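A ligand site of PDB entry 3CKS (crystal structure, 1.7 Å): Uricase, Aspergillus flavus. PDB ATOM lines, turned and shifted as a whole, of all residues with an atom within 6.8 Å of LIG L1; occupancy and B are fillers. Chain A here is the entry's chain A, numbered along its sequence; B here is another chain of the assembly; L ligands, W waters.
The backbone NH (N) of Thr 58 of chain B sits at hydrogen-bond distance from a nitrogen (N3) of LIG L1. N3 of LIG L1 sits at hydrogen-bond distance from OG1 of Thr 58 of chain B (3.3 Å). An oxygen (O1) of LIG L1 sits at hydrogen-bond distance from the guanidinium group (NH2) of Arg 177. N of Val 228 is in hydrogen-bond range of O1 of LIG L1 (2.9 Å). An oxygen (O2) of LIG L1 is in hydrogen-bond range of the side-chain amide nitrogen (NE2) of Gln 229. The side-chain amide nitrogen (ND2) of Asn 255 lies close to a nitrogen (N2) of LIG L1. O1 of LG2 L2 lies within hydrogen-bond range of OG1 of Thr 58 of chain B. O1 of LG2 L2 lies within hydrogen-bond range of ND2 of Asn 255 (3.0 Å).
Water W1 lies within hydrogen-bond range of a nitrogen (N5) of LIG L1 (2.7 Å) and the guanidinium group of Arg 177 (3.4 Å).
An oxygen (O1) of LG2 L2 lies close to a nitrogen (N5) of LIG L1.
The side-chain amino group of Lys 11 of chain B sits at hydrogen-bond distance from the side-chain hydroxyl of Thr 58 of chain B (2.9 Å). The backbone NH (N) of Arg 177 lies within hydrogen-bond range of the backbone carbonyl oxygen (O) of Ser 158, 2.9 Å away. The side-chain hydroxyl of Ser 227 sits close to the backbone NH of Gln 229, 3.4 Å away. O of Asn 255 lies within hydrogen-bond range of NE2 of His 257. The backbone NH (N) of Asn 255 lies within hydrogen-bond range of the backbone carbonyl oxygen (O) of Gly 287 (2.8 Å). The backbone carbonyl oxygen (O) of Ser 227 lies within hydrogen-bond range of the side-chain hydroxyl (OG) of Ser 225 (2.9 Å). The side-chain hydroxyl of Tyr 9 of chain B sits at hydrogen-bond distance from the backbone carbonyl oxygen of Val 56 of chain B (2.5 Å).
Phe 160 touches LIG L1 (CE2 to C2, 3.3 Å). CD2 of Leu 171 touches N4 of LIG L1 (3.8 Å). Ser 227 touches LIG L1. Tyr 9 of chain B touches LIG L1. CG2 of Ile 55 of chain B touches O2 of LIG L1 (3.5 Å). CA of Ala 57 of chain B touches N3 of LIG L1 (3.4 Å). Asp 59 of chain B touches LIG L1. Within 4 Å of LIG L1: Phe 160, Leu 171, Arg 177, Ser 227, Val 228, Gln 229, Asn 255, Tyr 9 of chain B, Ile 55 of chain B, Ala 57 of chain B, Thr 58 of chain B and Asp 59 of chain B. The nearest printed residue that does not touch LIG L1 is Ile 289 (4.04 Å).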
ATOM      1  N   SER A 158     -22.045 -23.723  25.953  1.00  0.00           N
ATOM      2  CA  SER A 158     -20.795 -23.018  25.970  1.00  0.00           C
ATOM      3  C   SER A 158     -19.833 -23.880  26.798  1.00  0.00           C
ATOM      4  O   SER A 158     -20.213 -24.440  27.847  1.00  0.00           O
ATOM      5  CB  SER A 158     -20.974 -21.656  26.648  1.00  0.00           C
ATOM      6  OG  SER A 158     -19.707 -21.060  26.864  1.00  0.00           O
ATOM      7  N   GLN A 159     -18.594 -23.990  26.327  1.00  0.00           N
ATOM      8  CA  GLN A 159     -17.574 -24.778  26.994  1.00  0.00           C
ATOM      9  C   GLN A 159     -16.302 -23.973  27.054  1.00  0.00           C
ATOM     10  O   GLN A 159     -16.121 -23.015  26.284  1.00  0.00           O
ATOM     11  CB  GLN A 159     -17.277 -26.074  26.187  1.00  0.00           C
ATOM     12  CG  GLN A 159     -18.500 -26.919  25.908  1.00  0.00           C
ATOM     13  CD  GLN A 159     -18.220 -28.156  25.065  1.00  0.00           C
ATOM     14  OE1 GLN A 159     -17.062 -28.519  24.819  1.00  0.00           O
ATOM     15  NE2 GLN A 159     -19.281 -28.816  24.622  1.00  0.00           N
ATOM     16  N   PHE A 160     -15.408 -24.391  27.932  1.00  0.00           N
ATOM     17  CA  PHE A 160     -14.083 -23.829  27.981  1.00  0.00           C
ATOM     18  C   PHE A 160     -13.129 -24.810  28.668  1.00  0.00           C
ATOM     19  O   PHE A 160     -13.081 -24.915  29.901  1.00  0.00           O
ATOM     20  CB  PHE A 160     -14.053 -22.393  28.595  1.00  0.00           C
ATOM     21  CG  PHE A 160     -12.754 -21.689  28.375  1.00  0.00           C
ATOM     22  CD1 PHE A 160     -12.338 -21.380  27.069  1.00  0.00           C
ATOM     23  CD2 PHE A 160     -11.933 -21.337  29.445  1.00  0.00           C
ATOM     24  CE1 PHE A 160     -11.121 -20.723  26.841  1.00  0.00           C
ATOM     25  CE2 PHE A 160     -10.713 -20.689  29.221  1.00  0.00           C
ATOM     26  CZ  PHE A 160     -10.289 -20.403  27.910  1.00  0.00           C
ATOM     27  N   PHE A 163      -7.255 -25.028  27.920  1.00  0.00           N
ATOM     28  CA  PHE A 163      -6.391 -23.862  28.034  1.00  0.00           C
ATOM     29  C   PHE A 163      -5.081 -24.168  28.785  1.00  0.00           C
ATOM     30  O   PHE A 163      -4.971 -25.183  29.470  1.00  0.00           O
ATOM     31  CB  PHE A 163      -7.136 -22.687  28.707  1.00  0.00           C
ATOM     32  CG  PHE A 163      -7.844 -23.074  29.964  1.00  0.00           C
ATOM     33  CD1 PHE A 163      -9.152 -23.537  29.911  1.00  0.00           C
ATOM     34  CD2 PHE A 163      -7.226 -22.937  31.216  1.00  0.00           C
ATOM     35  CE1 PHE A 163      -9.851 -23.891  31.060  1.00  0.00           C
ATOM     36  CE2 PHE A 163      -7.929 -23.298  32.376  1.00  0.00           C
ATOM     37  CZ  PHE A 163      -9.224 -23.782  32.295  1.00  0.00           C
ATOM     38  N   LEU A 171      -8.471 -21.949  37.474  1.00  0.00           N
ATOM     39  CA  LEU A 171      -9.737 -22.162  36.782  1.00  0.00           C
ATOM     40  C   LEU A 171      -9.927 -23.629  36.380  1.00  0.00           C
ATOM     41  O   LEU A 171      -9.027 -24.224  35.761  1.00  0.00           O
ATOM     42  CB  LEU A 171      -9.778 -21.285  35.535  1.00  0.00           C
ATOM     43  CG  LEU A 171     -11.052 -21.322  34.677  1.00  0.00           C
ATOM     44  CD1 LEU A 171     -12.237 -20.665  35.387  1.00  0.00           C
ATOM     45  CD2 LEU A 171     -10.793 -20.656  33.338  1.00  0.00           C
ATOM     46  N   ARG A 177     -21.246 -24.195  30.582  1.00  0.00           N
ATOM     47  CA  ARG A 177     -21.275 -22.958  31.367  1.00  0.00           C
ATOM     48  C   ARG A 177     -22.246 -21.981  30.735  1.00  0.00           C
ATOM     49  O   ARG A 177     -22.738 -22.186  29.632  1.00  0.00           O
ATOM     50  CB  ARG A 177     -19.877 -22.337  31.457  1.00  0.00           C
ATOM     51  CG  ARG A 177     -19.365 -21.904  30.110  1.00  0.00           C
ATOM     52  CD  ARG A 177     -17.990 -21.253  30.231  1.00  0.00           C
ATOM     53  NE  ARG A 177     -17.646 -20.625  28.939  1.00  0.00           N
ATOM     54  CZ  ARG A 177     -16.592 -19.852  28.693  1.00  0.00           C
ATOM     55  NH1 ARG A 177     -15.694 -19.574  29.646  1.00  0.00           N
ATOM     56  NH2 ARG A 177     -16.415 -19.356  27.455  1.00  0.00           N
ATOM     57  N   LEU A 179     -22.841 -18.359  29.092  1.00  0.00           N
ATOM     58  CA  LEU A 179     -22.085 -17.342  28.348  1.00  0.00           C
ATOM     59  C   LEU A 179     -22.968 -16.115  28.116  1.00  0.00           C
ATOM     60  O   LEU A 179     -24.055 -16.208  27.554  1.00  0.00           O
ATOM     61  CB  LEU A 179     -21.587 -17.898  27.011  1.00  0.00           C
ATOM     62  CG  LEU A 179     -20.892 -16.955  26.039  1.00  0.00           C
ATOM     63  CD1 LEU A 179     -19.639 -16.400  26.645  1.00  0.00           C
ATOM     64  CD2 LEU A 179     -20.557 -17.744  24.741  1.00  0.00           C
ATOM     65  N   SER A 225     -20.208 -23.407  21.757  1.00  0.00           N
ATOM     66  CA  SER A 225     -19.067 -22.528  21.734  1.00  0.00           C
ATOM     67  C   SER A 225     -17.861 -23.127  22.447  1.00  0.00           C
ATOM     68  O   SER A 225     -17.953 -23.564  23.593  1.00  0.00           O
ATOM     69  CB  SER A 225     -19.464 -21.174  22.376  1.00  0.00           C
ATOM     70  OG  SER A 225     -18.311 -20.384  22.573  1.00  0.00           O
ATOM     71  N   ALA A 226     -16.709 -23.120  21.776  1.00  0.00           N
ATOM     72  CA  ALA A 226     -15.490 -23.634  22.365  1.00  0.00           C
ATOM     73  C   ALA A 226     -14.789 -22.585  23.196  1.00  0.00           C
ATOM     74  O   ALA A 226     -13.895 -22.895  23.980  1.00  0.00           O
ATOM     75  CB  ALA A 226     -14.538 -24.103  21.257  1.00  0.00           C
ATOM     76  N   SER A 227     -15.160 -21.323  22.941  1.00  0.00           N
ATOM     77  CA  SER A 227     -14.595 -20.159  23.608  1.00  0.00           C
ATOM     78  C   SER A 227     -15.240 -18.926  23.002  1.00  0.00           C
ATOM     79  O   SER A 227     -15.851 -18.995  21.937  1.00  0.00           O
ATOM     80  CB  SER A 227     -13.072 -20.045  23.423  1.00  0.00           C
ATOM     81  OG  SER A 227     -12.714 -19.819  22.065  1.00  0.00           O
ATOM     82  N   VAL A 228     -15.061 -17.775  23.662  1.00  0.00           N
ATOM     83  CA  VAL A 228     -15.587 -16.578  23.081  1.00  0.00           C
ATOM     84  C   VAL A 228     -14.833 -16.311  21.781  1.00  0.00           C
ATOM     85  O   VAL A 228     -15.425 -15.898  20.796  1.00  0.00           O
ATOM     86  CB  VAL A 228     -15.427 -15.384  24.063  1.00  0.00           C
ATOM     87  CG1 VAL A 228     -15.848 -14.123  23.384  1.00  0.00           C
ATOM     88  CG2 VAL A 228     -16.297 -15.623  25.272  1.00  0.00           C
ATOM     89  N   GLN A 229     -13.515 -16.530  21.801  1.00  0.00           N
ATOM     90  CA  GLN A 229     -12.637 -16.328  20.633  1.00  0.00           C
ATOM     91  C   GLN A 229     -13.173 -17.082  19.401  1.00  0.00           C
ATOM     92  O   GLN A 229     -13.308 -16.525  18.299  1.00  0.00           O
ATOM     93  CB  GLN A 229     -11.227 -16.847  20.959  1.00  0.00           C
ATOM     94  CG  GLN A 229     -10.383 -15.962  21.922  1.00  0.00           C
ATOM     95  CD  GLN A 229     -10.611 -16.253  23.405  1.00  0.00           C
ATOM     96  OE1 GLN A 229     -11.667 -16.743  23.826  1.00  0.00           O
ATOM     97  NE2 GLN A 229      -9.589 -15.916  24.209  1.00  0.00           N
ATOM     98  N   ASN A 255     -16.668 -11.006  28.664  1.00  0.00           N
ATOM     99  CA  ASN A 255     -17.195 -12.274  29.119  1.00  0.00           C
ATOM    100  C   ASN A 255     -17.763 -11.979  30.507  1.00  0.00           C
ATOM    101  O   ASN A 255     -16.997 -11.823  31.435  1.00  0.00           O
ATOM    102  CB  ASN A 255     -16.048 -13.290  29.160  1.00  0.00           C
ATOM    103  CG  ASN A 255     -16.529 -14.716  29.418  1.00  0.00           C
ATOM    104  OD1 ASN A 255     -17.717 -14.967  29.612  1.00  0.00           O
ATOM    105  ND2 ASN A 255     -15.594 -15.666  29.451  1.00  0.00           N
ATOM    106  N   HIS A 257     -19.221 -12.858  33.718  1.00  0.00           N
ATOM    107  CA  HIS A 257     -19.200 -14.159  34.393  1.00  0.00           C
ATOM    108  C   HIS A 257     -20.389 -14.388  35.316  1.00  0.00           C
ATOM    109  O   HIS A 257     -20.790 -13.497  36.050  1.00  0.00           O
ATOM    110  CB  HIS A 257     -17.900 -14.322  35.179  1.00  0.00           C
ATOM    111  CG  HIS A 257     -16.674 -14.085  34.364  1.00  0.00           C
ATOM    112  ND1 HIS A 257     -16.334 -14.883  33.288  1.00  0.00           N
ATOM    113  CD2 HIS A 257     -15.709 -13.132  34.442  1.00  0.00           C
ATOM    114  CE1 HIS A 257     -15.189 -14.456  32.762  1.00  0.00           C
ATOM    115  NE2 HIS A 257     -14.809 -13.385  33.435  1.00  0.00           N
ATOM    116  N   GLY A 287     -13.756 -10.869  31.608  1.00  0.00           N
ATOM    117  CA  GLY A 287     -12.894 -11.088  30.457  1.00  0.00           C
ATOM    118  C   GLY A 287     -13.209 -10.073  29.376  1.00  0.00           C
ATOM    119  O   GLY A 287     -14.328  -9.532  29.303  1.00  0.00           O
ATOM    120  N   ILE A 289     -12.434  -9.791  25.185  1.00  0.00           N
ATOM    121  CA  ILE A 289     -11.842 -10.503  24.058  1.00  0.00           C
ATOM    122  C   ILE A 289     -12.081  -9.685  22.799  1.00  0.00           C
ATOM    123  O   ILE A 289     -13.227  -9.302  22.539  1.00  0.00           O
ATOM    124  CB  ILE A 289     -12.489 -11.919  23.886  1.00  0.00           C
ATOM    125  CG1 ILE A 289     -12.742 -12.619  25.249  1.00  0.00           C
ATOM    126  CG2 ILE A 289     -11.662 -12.739  22.881  1.00  0.00           C
ATOM    127  CD1 ILE A 289     -11.553 -12.929  26.063  1.00  0.00           C
ATOM    128  N   TYR B   9      -6.673 -10.080  24.041  1.00  0.00           N
ATOM    129  CA  TYR B   9      -7.676 -10.583  24.977  1.00  0.00           C
ATOM    130  C   TYR B   9      -7.064 -10.495  26.400  1.00  0.00           C
ATOM    131  O   TYR B   9      -5.840 -10.453  26.575  1.00  0.00           O
ATOM    132  CB  TYR B   9      -8.110 -12.026  24.625  1.00  0.00           C
ATOM    133  CG  TYR B   9      -7.155 -13.014  25.198  1.00  0.00           C
ATOM    134  CD1 TYR B   9      -5.883 -13.172  24.650  1.00  0.00           C
ATOM    135  CD2 TYR B   9      -7.475 -13.718  26.363  1.00  0.00           C
ATOM    136  CE1 TYR B   9      -4.952 -14.024  25.230  1.00  0.00           C
ATOM    137  CE2 TYR B   9      -6.568 -14.566  26.947  1.00  0.00           C
ATOM    138  CZ  TYR B   9      -5.305 -14.704  26.374  1.00  0.00           C
ATOM    139  OH  TYR B   9      -4.389 -15.533  26.966  1.00  0.00           O
ATOM    140  N   GLY B  10      -7.924 -10.484  27.411  1.00  0.00           N
ATOM    141  CA  GLY B  10      -7.422 -10.440  28.782  1.00  0.00           C
ATOM    142  C   GLY B  10      -8.515 -10.151  29.775  1.00  0.00           C
ATOM    143  O   GLY B  10      -9.648 -10.545  29.579  1.00  0.00           O
ATOM    144  N   LYS B  11      -8.165  -9.456  30.864  1.00  0.00           N
ATOM    145  CA  LYS B  11      -9.130  -9.253  31.967  1.00  0.00           C
ATOM    146  C   LYS B  11      -9.257  -7.756  32.199  1.00  0.00           C
ATOM    147  O   LYS B  11      -8.240  -7.065  32.251  1.00  0.00           O
ATOM    148  CB  LYS B  11      -8.636  -9.938  33.247  1.00  0.00           C
ATOM    149  CG  LYS B  11      -9.760 -10.201  34.268  1.00  0.00           C
ATOM    150  CD  LYS B  11     -10.790 -11.215  33.700  1.00  0.00           C
ATOM    151  CE  LYS B  11     -11.140 -12.309  34.665  1.00  0.00           C
ATOM    152  NZ  LYS B  11     -11.949 -13.388  33.956  1.00  0.00           N
ATOM    153  N   ASN B  52      -7.498 -23.984  22.250  1.00  0.00           N
ATOM    154  CA  ASN B  52      -7.334 -23.251  23.518  1.00  0.00           C
ATOM    155  C   ASN B  52      -5.948 -23.391  24.161  1.00  0.00           C
ATOM    156  O   ASN B  52      -5.665 -22.759  25.172  1.00  0.00           O
ATOM    157  CB  ASN B  52      -8.465 -23.566  24.508  1.00  0.00           C
ATOM    158  CG  ASN B  52      -9.831 -23.106  24.002  1.00  0.00           C
ATOM    159  OD1 ASN B  52      -9.934 -22.185  23.189  1.00  0.00           O
ATOM    160  ND2 ASN B  52     -10.885 -23.736  24.495  1.00  0.00           N
ATOM    161  N   ILE B  55      -4.116 -20.273  24.959  1.00  0.00           N
ATOM    162  CA  ILE B  55      -4.755 -19.292  25.829  1.00  0.00           C
ATOM    163  C   ILE B  55      -4.295 -19.388  27.284  1.00  0.00           C
ATOM    164  O   ILE B  55      -4.500 -20.413  27.934  1.00  0.00           O
ATOM    165  CB  ILE B  55      -6.289 -19.347  25.753  1.00  0.00           C
ATOM    166  CG1 ILE B  55      -6.774 -19.046  24.328  1.00  0.00           C
ATOM    167  CG2 ILE B  55      -6.939 -18.324  26.766  1.00  0.00           C
ATOM    168  CD1 ILE B  55      -6.401 -17.591  23.800  1.00  0.00           C
ATOM    169  N   VAL B  56      -3.664 -18.312  27.740  1.00  0.00           N
ATOM    170  CA  VAL B  56      -3.484 -18.084  29.167  1.00  0.00           C
ATOM    171  C   VAL B  56      -4.855 -17.563  29.598  1.00  0.00           C
ATOM    172  O   VAL B  56      -5.254 -16.486  29.128  1.00  0.00           O
ATOM    173  CB  VAL B  56      -2.391 -17.026  29.410  1.00  0.00           C
ATOM    174  CG1 VAL B  56      -2.289 -16.667  30.904  1.00  0.00           C
ATOM    175  CG2 VAL B  56      -1.023 -17.524  28.859  1.00  0.00           C
ATOM    176  N   ALA B  57      -5.568 -18.312  30.450  1.00  0.00           N
ATOM    177  CA  ALA B  57      -6.966 -17.979  30.754  1.00  0.00           C
ATOM    178  C   ALA B  57      -7.043 -16.597  31.391  1.00  0.00           C
ATOM    179  O   ALA B  57      -6.145 -16.197  32.134  1.00  0.00           O
ATOM    180  CB  ALA B  57      -7.603 -19.063  31.654  1.00  0.00           C
ATOM    181  N   THR B  58      -8.137 -15.874  31.114  1.00  0.00           N
ATOM    182  CA  THR B  58      -8.257 -14.521  31.652  1.00  0.00           C
ATOM    183  C   THR B  58      -8.329 -14.603  33.177  1.00  0.00           C
ATOM    184  O   THR B  58      -7.834 -13.709  33.853  1.00  0.00           O
ATOM    185  CB  THR B  58      -9.477 -13.757  31.098  1.00  0.00           C
ATOM    186  OG1 THR B  58     -10.686 -14.364  31.545  1.00  0.00           O
ATOM    187  CG2 THR B  58      -9.452 -13.764  29.547  1.00  0.00           C
ATOM    188  N   ASP B  59      -8.918 -15.676  33.695  1.00  0.00           N
ATOM    189  CA  ASP B  59      -8.911 -15.933  35.157  1.00  0.00           C
ATOM    190  C   ASP B  59      -7.499 -16.018  35.723  1.00  0.00           C
ATOM    191  O   ASP B  59      -7.220 -15.526  36.813  1.00  0.00           O
ATOM    192  CB  ASP B  59      -9.649 -17.233  35.471  1.00  0.00           C
ATOM    193  CG  ASP B  59      -9.881 -17.402  36.969  1.00  0.00           C
ATOM    194  OD1 ASP B  59     -10.787 -16.727  37.490  1.00  0.00           O
ATOM    195  OD2 ASP B  59      -9.124 -18.147  37.619  1.00  0.00           O
ATOM    196  N   SER B  60      -6.585 -16.641  34.961  1.00  0.00           N
ATOM    197  CA  SER B  60      -5.177 -16.661  35.373  1.00  0.00           C
ATOM    198  C   SER B  60      -4.512 -15.302  35.338  1.00  0.00           C
ATOM    199  O   SER B  60      -3.650 -14.999  36.153  1.00  0.00           O
ATOM    200  CB  SER B  60      -4.377 -17.670  34.512  1.00  0.00           C
ATOM    201  OG  SER B  60      -5.059 -18.916  34.549  1.00  0.00           O
HETATM  202  N1  LIG L   1     -12.087 -17.251  26.723  1.00  0.00           N
HETATM  203  C1  LIG L   1     -13.238 -17.753  27.221  1.00  0.00           C
HETATM  204  O1  LIG L   1     -14.169 -17.947  26.397  1.00  0.00           O
HETATM  205  N2  LIG L   1     -13.402 -18.045  28.554  1.00  0.00           N
HETATM  206  C2  LIG L   1     -12.345 -17.827  29.375  1.00  0.00           C
HETATM  207  C3  LIG L   1     -11.106 -17.289  28.907  1.00  0.00           C
HETATM  208  C4  LIG L   1     -10.998 -17.008  27.474  1.00  0.00           C
HETATM  209  O2  LIG L   1      -9.952 -16.519  27.013  1.00  0.00           O
HETATM  210  N3  LIG L   1     -10.210 -17.176  29.958  1.00  0.00           N
HETATM  211  N4  LIG L   1     -10.964 -17.643  31.061  1.00  0.00           N
HETATM  212  N5  LIG L   1     -12.276 -18.049  30.741  1.00  0.00           N
HETATM  213  O1  LG2 L   2     -12.814 -14.760  30.287  1.00  0.00           O
HETATM  214  O2  LG2 L   2     -13.020 -14.048  29.343  1.00  0.00           O
HETATM  215  O   HOH W   1     -14.239 -18.483  32.522  1.00  0.00           O
